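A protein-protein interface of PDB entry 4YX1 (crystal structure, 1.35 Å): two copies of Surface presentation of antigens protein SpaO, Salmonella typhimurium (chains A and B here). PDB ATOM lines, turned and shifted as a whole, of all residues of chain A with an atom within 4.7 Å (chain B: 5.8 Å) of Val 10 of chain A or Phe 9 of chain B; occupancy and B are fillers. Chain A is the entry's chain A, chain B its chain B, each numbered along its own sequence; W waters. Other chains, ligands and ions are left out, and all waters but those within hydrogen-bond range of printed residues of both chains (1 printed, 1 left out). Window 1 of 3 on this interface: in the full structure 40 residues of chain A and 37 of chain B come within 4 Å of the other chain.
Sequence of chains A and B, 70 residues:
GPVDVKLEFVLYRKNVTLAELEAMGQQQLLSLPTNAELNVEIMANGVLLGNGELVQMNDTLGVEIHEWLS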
ATOM      1  N   GLU A   8       4.968  19.392  34.238  1.00  0.00           N
ATOM      2  CA  GLU A   8       5.409  20.244  33.143  1.00  0.00           C
ATOM      3  C   GLU A   8       6.379  19.518  32.236  1.00  0.00           C
ATOM      4  O   GLU A   8       7.232  18.738  32.703  1.00  0.00           O
ATOM      5  CB  GLU A   8       6.093  21.504  33.662  1.00  0.00           C
ATOM      6  CG  GLU A   8       5.222  22.441  34.466  1.00  0.00           C
ATOM      7  CD  GLU A   8       5.948  23.744  34.750  1.00  0.00           C
ATOM      8  OE1 GLU A   8       7.193  23.728  34.705  1.00  0.00           O
ATOM      9  OE2 GLU A   8       5.292  24.777  34.999  1.00  0.00           O
ATOM     10  N   PHE A   9       6.252  19.786  30.941  1.00  0.00           N
ATOM     11  CA  PHE A   9       7.247  19.386  29.958  1.00  0.00           C
ATOM     12  C   PHE A   9       7.960  20.659  29.564  1.00  0.00           C
ATOM     13  O   PHE A   9       7.353  21.538  28.949  1.00  0.00           O
ATOM     14  CB  PHE A   9       6.610  18.695  28.748  1.00  0.00           C
ATOM     15  CG  PHE A   9       5.968  17.394  29.078  1.00  0.00           C
ATOM     16  CD1 PHE A   9       4.669  17.350  29.564  1.00  0.00           C
ATOM     17  CD2 PHE A   9       6.673  16.215  28.955  1.00  0.00           C
ATOM     18  CE1 PHE A   9       4.077  16.151  29.890  1.00  0.00           C
ATOM     19  CE2 PHE A   9       6.086  15.004  29.278  1.00  0.00           C
ATOM     20  CZ  PHE A   9       4.787  14.971  29.749  1.00  0.00           C
ATOM     21  N   VAL A  10       9.224  20.777  29.953  1.00  0.00           N
ATOM     22  CA  VAL A  10       9.945  22.033  29.813  1.00  0.00           C
ATOM     23  C   VAL A  10      10.986  21.922  28.713  1.00  0.00           C
ATOM     24  O   VAL A  10      11.851  21.051  28.738  1.00  0.00           O
ATOM     25  CB  VAL A  10      10.604  22.438  31.157  1.00  0.00           C
ATOM     26  CG1 VAL A  10      11.443  23.686  31.009  1.00  0.00           C
ATOM     27  CG2 VAL A  10       9.533  22.638  32.226  1.00  0.00           C
ATOM     28  N   LEU A  11      10.871  22.783  27.717  1.00  0.00           N
ATOM     29  CA  LEU A  11      11.771  22.737  26.579  1.00  0.00           C
ATOM     30  C   LEU A  11      13.118  23.357  26.938  1.00  0.00           C
ATOM     31  O   LEU A  11      14.161  22.925  26.449  1.00  0.00           O
ATOM     32  CB  LEU A  11      11.145  23.455  25.378  1.00  0.00           C
ATOM     33  CG  LEU A  11      11.938  23.467  24.079  1.00  0.00           C
ATOM     34  CD1 LEU A  11      12.323  22.052  23.712  1.00  0.00           C
ATOM     35  CD2 LEU A  11      11.073  24.044  23.007  1.00  0.00           C
ATOM     36  N   TYR A  12      13.091  24.367  27.796  1.00  0.00           N
ATOM     37  CA  TYR A  12      14.304  25.054  28.170  1.00  0.00           C
ATOM     38  C   TYR A  12      14.063  25.795  29.465  1.00  0.00           C
ATOM     39  O   TYR A  12      13.016  26.403  29.649  1.00  0.00           O
ATOM     40  CB  TYR A  12      14.755  25.998  27.042  1.00  0.00           C
ATOM     41  CG  TYR A  12      16.062  26.692  27.339  1.00  0.00           C
ATOM     42  CD1 TYR A  12      17.233  25.968  27.534  1.00  0.00           C
ATOM     43  CD2 TYR A  12      16.119  28.072  27.452  1.00  0.00           C
ATOM     44  CE1 TYR A  12      18.429  26.609  27.822  1.00  0.00           C
ATOM     45  CE2 TYR A  12      17.303  28.720  27.728  1.00  0.00           C
ATOM     46  CZ  TYR A  12      18.454  27.985  27.922  1.00  0.00           C
ATOM     47  OH  TYR A  12      19.632  28.636  28.203  1.00  0.00           O
ATOM     48  N   ARG A  13      15.007  25.724  30.391  1.00  0.00           N
ATOM     49  CA  ARG A  13      14.926  26.555  31.566  1.00  0.00           C
ATOM     50  C   ARG A  13      16.287  27.095  31.925  1.00  0.00           C
ATOM     51  O   ARG A  13      17.317  26.512  31.588  1.00  0.00           O
ATOM     52  CB  ARG A  13      14.327  25.799  32.727  1.00  0.00           C
ATOM     53  CG  ARG A  13      15.023  24.522  33.021  1.00  0.00           C
ATOM     54  CD  ARG A  13      14.567  23.963  34.369  1.00  0.00           C
ATOM     55  NE  ARG A  13      15.174  22.658  34.586  1.00  0.00           N
ATOM     56  CZ  ARG A  13      15.520  22.168  35.768  1.00  0.00           C
ATOM     57  NH1 ARG A  13      15.305  22.861  36.881  1.00  0.00           N
ATOM     58  NH2 ARG A  13      16.085  20.977  35.827  1.00  0.00           N
ATOM     59  N   MET A  24      14.570  40.053  26.667  1.00  0.00           N
ATOM     60  CA  MET A  24      13.759  39.041  26.009  1.00  0.00           C
ATOM     61  C   MET A  24      12.373  39.573  25.661  1.00  0.00           C
ATOM     62  O   MET A  24      11.830  39.288  24.590  1.00  0.00           O
ATOM     63  CB  MET A  24      13.639  37.816  26.905  1.00  0.00           C
ATOM     64  CG  MET A  24      12.440  36.926  26.616  1.00  0.00           C
ATOM     65  SD  MET A  24      12.433  35.467  27.881  1.00  0.00           S
ATOM     66  CE  MET A  24      14.427  35.350  27.890  1.00  0.00           C
ATOM     67  N   LEU A  32      16.104  29.465  20.879  1.00  0.00           N
ATOM     68  CA  LEU A  32      16.500  28.581  21.965  1.00  0.00           C
ATOM     69  C   LEU A  32      17.899  28.058  21.688  1.00  0.00           C
ATOM     70  O   LEU A  32      18.345  28.074  20.537  1.00  0.00           O
ATOM     71  CB  LEU A  32      15.505  27.436  22.117  1.00  0.00           C
ATOM     72  CG  LEU A  32      14.095  27.901  22.477  1.00  0.00           C
ATOM     73  CD1 LEU A  32      13.177  26.722  22.568  1.00  0.00           C
ATOM     74  CD2 LEU A  32      14.101  28.669  23.796  1.00  0.00           C
ATOM     75  N   ASN A  39      16.865  17.832  25.388  1.00  0.00           N
ATOM     76  CA  ASN A  39      16.776  17.824  26.838  1.00  0.00           C
ATOM     77  C   ASN A  39      15.456  18.422  27.291  1.00  0.00           C
ATOM     78  O   ASN A  39      15.420  19.392  28.059  1.00  0.00           O
ATOM     79  CB  ASN A  39      17.948  18.589  27.461  1.00  0.00           C
ATOM     80  CG  ASN A  39      18.022  18.419  28.973  1.00  0.00           C
ATOM     81  OD1 ASN A  39      17.659  17.375  29.515  1.00  0.00           O
ATOM     82  ND2 ASN A  39      18.464  19.458  29.658  1.00  0.00           N
ATOM     83  N   VAL A  40      14.366  17.847  26.807  1.00  0.00           N
ATOM     84  CA  VAL A  40      13.057  18.193  27.336  1.00  0.00           C
ATOM     85  C   VAL A  40      12.968  17.630  28.734  1.00  0.00           C
ATOM     86  O   VAL A  40      13.217  16.455  28.949  1.00  0.00           O
ATOM     87  CB  VAL A  40      11.918  17.649  26.476  1.00  0.00           C
ATOM     88  CG1 VAL A  40      10.566  18.001  27.110  1.00  0.00           C
ATOM     89  CG2 VAL A  40      12.030  18.222  25.069  1.00  0.00           C
ATOM     90  N   GLU A  41      12.674  18.476  29.700  1.00  0.00           N
ATOM     91  CA  GLU A  41      12.667  18.052  31.080  1.00  0.00           C
ATOM     92  C   GLU A  41      11.251  17.855  31.576  1.00  0.00           C
ATOM     93  O   GLU A  41      10.368  18.673  31.311  1.00  0.00           O
ATOM     94  CB  GLU A  41      13.406  19.072  31.924  1.00  0.00           C
ATOM     95  CG  GLU A  41      14.887  19.095  31.605  1.00  0.00           C
ATOM     96  CD  GLU A  41      15.636  20.101  32.431  1.00  0.00           C
ATOM     97  OE1 GLU A  41      15.331  21.300  32.305  1.00  0.00           O
ATOM     98  OE2 GLU A  41      16.526  19.701  33.209  1.00  0.00           O
ATOM     99  N   MET A  43       8.982  17.792  34.730  1.00  0.00           N
ATOM    100  CA  MET A  43       8.953  18.333  36.084  1.00  0.00           C
ATOM    101  C   MET A  43       7.663  17.949  36.774  1.00  0.00           C
ATOM    102  O   MET A  43       6.597  17.978  36.173  1.00  0.00           O
ATOM    103  CB  MET A  43       9.049  19.862  36.071  1.00  0.00           C
ATOM    104  CG  MET A  43      10.040  20.448  35.104  1.00  0.00           C
ATOM    105  SD  MET A  43      11.871  20.208  35.680  1.00  0.00           S
ATOM    106  CE  MET A  43      11.903  21.303  37.275  1.00  0.00           C
ATOM    107  N   LEU B   7      13.452  31.084  34.748  1.00  0.00           N
ATOM    108  CA  LEU B   7      12.728  31.144  33.480  1.00  0.00           C
ATOM    109  C   LEU B   7      12.500  29.754  32.898  1.00  0.00           C
ATOM    110  O   LEU B   7      13.418  28.938  32.863  1.00  0.00           O
ATOM    111  CB  LEU B   7      13.516  31.999  32.490  1.00  0.00           C
ATOM    112  CG  LEU B   7      12.991  32.114  31.062  1.00  0.00           C
ATOM    113  CD1 LEU B   7      11.666  32.855  31.039  1.00  0.00           C
ATOM    114  CD2 LEU B   7      14.011  32.826  30.191  1.00  0.00           C
ATOM    115  N   GLU B   8      11.286  29.490  32.423  1.00  0.00           N
ATOM    116  CA  GLU B   8      10.964  28.232  31.757  1.00  0.00           C
ATOM    117  C   GLU B   8      10.181  28.460  30.481  1.00  0.00           C
ATOM    118  O   GLU B   8       9.290  29.313  30.428  1.00  0.00           O
ATOM    119  CB  GLU B   8      10.134  27.323  32.659  1.00  0.00           C
ATOM    120  CG  GLU B   8      10.824  26.808  33.903  1.00  0.00           C
ATOM    121  CD  GLU B   8       9.947  25.812  34.642  1.00  0.00           C
ATOM    122  OE1 GLU B   8       8.715  25.797  34.397  1.00  0.00           O
ATOM    123  OE2 GLU B   8      10.484  25.033  35.446  1.00  0.00           O
ATOM    124  N   PHE B   9      10.505  27.691  29.453  1.00  0.00           N
ATOM    125  CA  PHE B   9       9.676  27.585  28.258  1.00  0.00           C
ATOM    126  C   PHE B   9       8.947  26.262  28.355  1.00  0.00           C
ATOM    127  O   PHE B   9       9.569  25.201  28.271  1.00  0.00           O
ATOM    128  CB  PHE B   9      10.515  27.675  26.985  1.00  0.00           C
ATOM    129  CG  PHE B   9      11.175  29.004  26.804  1.00  0.00           C
ATOM    130  CD1 PHE B   9      12.355  29.302  27.462  1.00  0.00           C
ATOM    131  CD2 PHE B   9      10.608  29.969  25.983  1.00  0.00           C
ATOM    132  CE1 PHE B   9      12.959  30.531  27.309  1.00  0.00           C
ATOM    133  CE2 PHE B   9      11.208  31.199  25.824  1.00  0.00           C
ATOM    134  CZ  PHE B   9      12.388  31.476  26.486  1.00  0.00           C
ATOM    135  N   VAL B  10       7.644  26.328  28.588  1.00  0.00           N
ATOM    136  CA  VAL B  10       6.848  25.155  28.924  1.00  0.00           C
ATOM    137  C   VAL B  10       6.061  24.709  27.709  1.00  0.00           C
ATOM    138  O   VAL B  10       5.224  25.445  27.197  1.00  0.00           O
ATOM    139  CB  VAL B  10       5.886  25.458  30.100  1.00  0.00           C
ATOM    140  CG1 VAL B  10       5.018  24.250  30.419  1.00  0.00           C
ATOM    141  CG2 VAL B  10       6.686  25.918  31.329  1.00  0.00           C
ATOM    142  N   LEU B  11       6.352  23.518  27.222  1.00  0.00           N
ATOM    143  CA  LEU B  11       5.685  23.006  26.042  1.00  0.00           C
ATOM    144  C   LEU B  11       4.279  22.547  26.381  1.00  0.00           C
ATOM    145  O   LEU B  11       3.345  22.735  25.597  1.00  0.00           O
ATOM    146  CB  LEU B  11       6.496  21.874  25.433  1.00  0.00           C
ATOM    147  CG  LEU B  11       5.978  21.255  24.146  1.00  0.00           C
ATOM    148  CD1 LEU B  11       5.713  22.315  23.096  1.00  0.00           C
ATOM    149  CD2 LEU B  11       7.039  20.302  23.669  1.00  0.00           C
ATOM    150  N   TYR B  12       4.122  21.976  27.569  1.00  0.00           N
ATOM    151  CA  TYR B  12       2.827  21.505  27.996  1.00  0.00           C
ATOM    152  C   TYR B  12       2.810  21.387  29.501  1.00  0.00           C
ATOM    153  O   TYR B  12       3.805  21.012  30.123  1.00  0.00           O
ATOM    154  CB  TYR B  12       2.492  20.161  27.327  1.00  0.00           C
ATOM    155  CG  TYR B  12       1.119  19.664  27.695  1.00  0.00           C
ATOM    156  CD1 TYR B  12      -0.010  20.422  27.398  1.00  0.00           C
ATOM    157  CD2 TYR B  12       0.943  18.451  28.345  1.00  0.00           C
ATOM    158  CE1 TYR B  12      -1.276  19.988  27.742  1.00  0.00           C
ATOM    159  CE2 TYR B  12      -0.318  18.004  28.688  1.00  0.00           C
ATOM    160  CZ  TYR B  12      -1.422  18.777  28.381  1.00  0.00           C
ATOM    161  OH  TYR B  12      -2.684  18.341  28.717  1.00  0.00           O
ATOM    162  N   VAL B  40       3.159  27.313  23.577  1.00  0.00           N
ATOM    163  CA  VAL B  40       4.336  27.300  24.427  1.00  0.00           C
ATOM    164  C   VAL B  40       4.152  28.417  25.430  1.00  0.00           C
ATOM    165  O   VAL B  40       3.866  29.545  25.047  1.00  0.00           O
ATOM    166  CB  VAL B  40       5.633  27.505  23.623  1.00  0.00           C
ATOM    167  CG1 VAL B  40       6.843  27.587  24.556  1.00  0.00           C
ATOM    168  CG2 VAL B  40       5.789  26.396  22.581  1.00  0.00           C
ATOM    169  N   GLU B  41       4.272  28.115  26.708  1.00  0.00           N
ATOM    170  CA  GLU B  41       4.111  29.150  27.724  1.00  0.00           C
ATOM    171  C   GLU B  41       5.452  29.579  28.272  1.00  0.00           C
ATOM    172  O   GLU B  41       6.295  28.747  28.612  1.00  0.00           O
ATOM    173  CB  GLU B  41       3.198  28.648  28.835  1.00  0.00           C
ATOM    174  CG  GLU B  41       1.785  28.426  28.342  1.00  0.00           C
ATOM    175  CD  GLU B  41       0.896  27.828  29.398  1.00  0.00           C
ATOM    176  OE1 GLU B  41       1.180  26.694  29.832  1.00  0.00           O
ATOM    177  OE2 GLU B  41      -0.077  28.498  29.802  1.00  0.00           O
ATOM    178  N   ILE B  42       5.659  30.876  28.344  1.00  0.00           N
ATOM    179  CA  ILE B  42       6.877  31.422  28.889  1.00  0.00           C
ATOM    180  C   ILE B  42       6.566  31.842  30.307  1.00  0.00           C
ATOM    181  O   ILE B  42       5.674  32.664  30.536  1.00  0.00           O
ATOM    182  CB  ILE B  42       7.385  32.615  28.069  1.00  0.00           C
ATOM    183  CG1 ILE B  42       7.524  32.223  26.589  1.00  0.00           C
ATOM    184  CG2 ILE B  42       8.698  33.137  28.641  1.00  0.00           C
ATOM    185  CD1 ILE B  42       6.303  32.483  25.726  1.00  0.00           C
ATOM    186  N   MET B  43       7.277  31.248  31.259  1.00  0.00           N
ATOM    187  CA  MET B  43       6.997  31.442  32.666  1.00  0.00           C
ATOM    188  C   MET B  43       8.254  31.810  33.426  1.00  0.00           C
ATOM    189  O   MET B  43       9.345  31.390  33.068  1.00  0.00           O
ATOM    190  CB  MET B  43       6.371  30.180  33.234  1.00  0.00           C
ATOM    191  CG  MET B  43       5.166  29.759  32.414  1.00  0.00           C
ATOM    192  SD  MET B  43       4.066  28.444  33.274  1.00  0.00           S
ATOM    193  CE  MET B  43       3.473  29.567  34.750  1.00  0.00           C
ATOM    194  N   VAL B  63      10.953  30.282  19.569  1.00  0.00           N
ATOM    195  CA  VAL B  63       9.596  30.511  20.012  1.00  0.00           C
ATOM    196  C   VAL B  63       9.110  31.840  19.451  1.00  0.00           C
ATOM    197  O   VAL B  63       9.642  32.909  19.786  1.00  0.00           O
ATOM    198  CB  VAL B  63       9.493  30.497  21.545  1.00  0.00           C
ATOM    199  CG1 VAL B  63       8.056  30.738  21.975  1.00  0.00           C
ATOM    200  CG2 VAL B  63       9.980  29.167  22.080  1.00  0.00           C
HETATM  201  O   HOH W   1       8.951  23.678  37.149  1.00  0.00           O
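The side-chain carboxylate of Glu 8 of chain B lies close to the side-chain carboxylate of Glu 8 of chain A (2.6 Å).
N of Leu 11 of chain B lies within hydrogen-bond range of O of Phe 9 of chain A, at 2.8 Å.
O of Tyr 12 of chain B sits at hydrogen-bond distance from N of Phe 9 of chain A (2.9 Å).
N of Leu 11 of chain A lies within hydrogen-bond range of O of Phe 9 of chain B, 2.8 Å away.
The backbone carbonyl oxygen of Tyr 12 of chain A sits at hydrogen-bond distance from the backbone NH of Phe 9 of chain B, 2.8 Å away.
N of Met 43 of chain A sits at hydrogen-bond distance from O of Glu 8 of chain A (2.8 Å).
The backbone NH (N) of Val 10 of chain A is in hydrogen-bond range of the backbone carbonyl oxygen (O) of Glu 41 of chain A.
NE of Arg 13 of chain A lies within salt-bridge range of OE1 of Glu 41 of chain A, 2.7 Å away.
The backbone carbonyl oxygen (O) of Met 43 of chain B sits at hydrogen-bond distance from the backbone NH (N) of Glu 8 of chain B, at 2.8 Å.
N of Val 10 of chain B is in hydrogen-bond range of O of Glu 41 of chain B, 2.8 Å away.
Among the printed residues, merely in contact across the chains: Arg 13 of chain A with Leu 7 of chain B, Met 24 of chain A with Leu 7 of chain B, Tyr 12 of chain A with Glu 8 of chain B, Glu 8 of chain A with Tyr 12 of chain B, Val 10 of chain A with Phe 9 of chain B, Phe 9 of chain A with Val 10 of chain B, Arg 13 of chain A with Glu 8 of chain B and Val 10 of chain A with Glu 8 of chain B.
Val 10 of chain A touches just these residues of chain B: Glu 8 and Phe 9.
Phe 9 of chain B touches three residues of chain A.
Printed residues of chain B within 4 Å of Glu 8 of chain A: Glu 8 and Tyr 12.
Printed residues of chain B within 4 Å of Arg 13 of chain A: Leu 7 and Glu 8.
Of the printed residues of chain A, Tyr 12 of chain B touches Glu 8 (3.5 Å) and Phe 9 (2.9 Å).
Met 43 of chain A touches none of the printed residues of chain B.
Val 63 of chain B touches none of the printed residues of chain A.
The nearest residue of chain B that does not touch Val 10 of chain A is Val 10 of chain B (4.4 Å).
The nearest printed residue of chain B that does not touch Met 24 of chain A is Phe 9 of chain B (4.2 Å).
Of the 12 printed residues of chain A, 7 touch a printed residue of chain B.
Hydrophobic or aromatic side chains of chain A that line the printed part of chain B: Phe 9, Val 10, Leu 11, Tyr 12 and Met 24.
Printed residues of chain B that touch a printed residue of chain A: Leu 7, Glu 8, Phe 9, Val 10, Leu 11 and Tyr 12.
Hydrophobic or aromatic side chains of chain B within 4 Å of the printed part of chain A: Leu 7, Phe 9, Val 10 and Leu 11.
Among the printed residues, 13 pairs touch across the chains.
Among the printed residues, no Asp or Glu carboxylate lies within 4 Å of a Lys or Arg side-chain nitrogen of the other chain.
Glu 8 of chain A touches Tyr 12 of chain B, and with the chains exchanged Tyr 12 of chain A touches Glu 8 of chain B.
Phe 9 of chain A touches Val 10 of chain B, and with the chains exchanged Val 10 of chain A touches Phe 9 of chain B.
Phe 9 of chain A touches Leu 11 of chain B, and with the chains exchanged Leu 11 of chain A touches Phe 9 of chain B.
Phe 9 of chain A touches Tyr 12 of chain B, and with the chains exchanged Tyr 12 of chain A touches Phe 9 of chain B.
8 positions are printed for both chains.
Water W1 lies within hydrogen-bond range of the side-chain carboxylate of Glu 8 of chain B and the side-chain carboxylate of Glu 8 of chain A.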
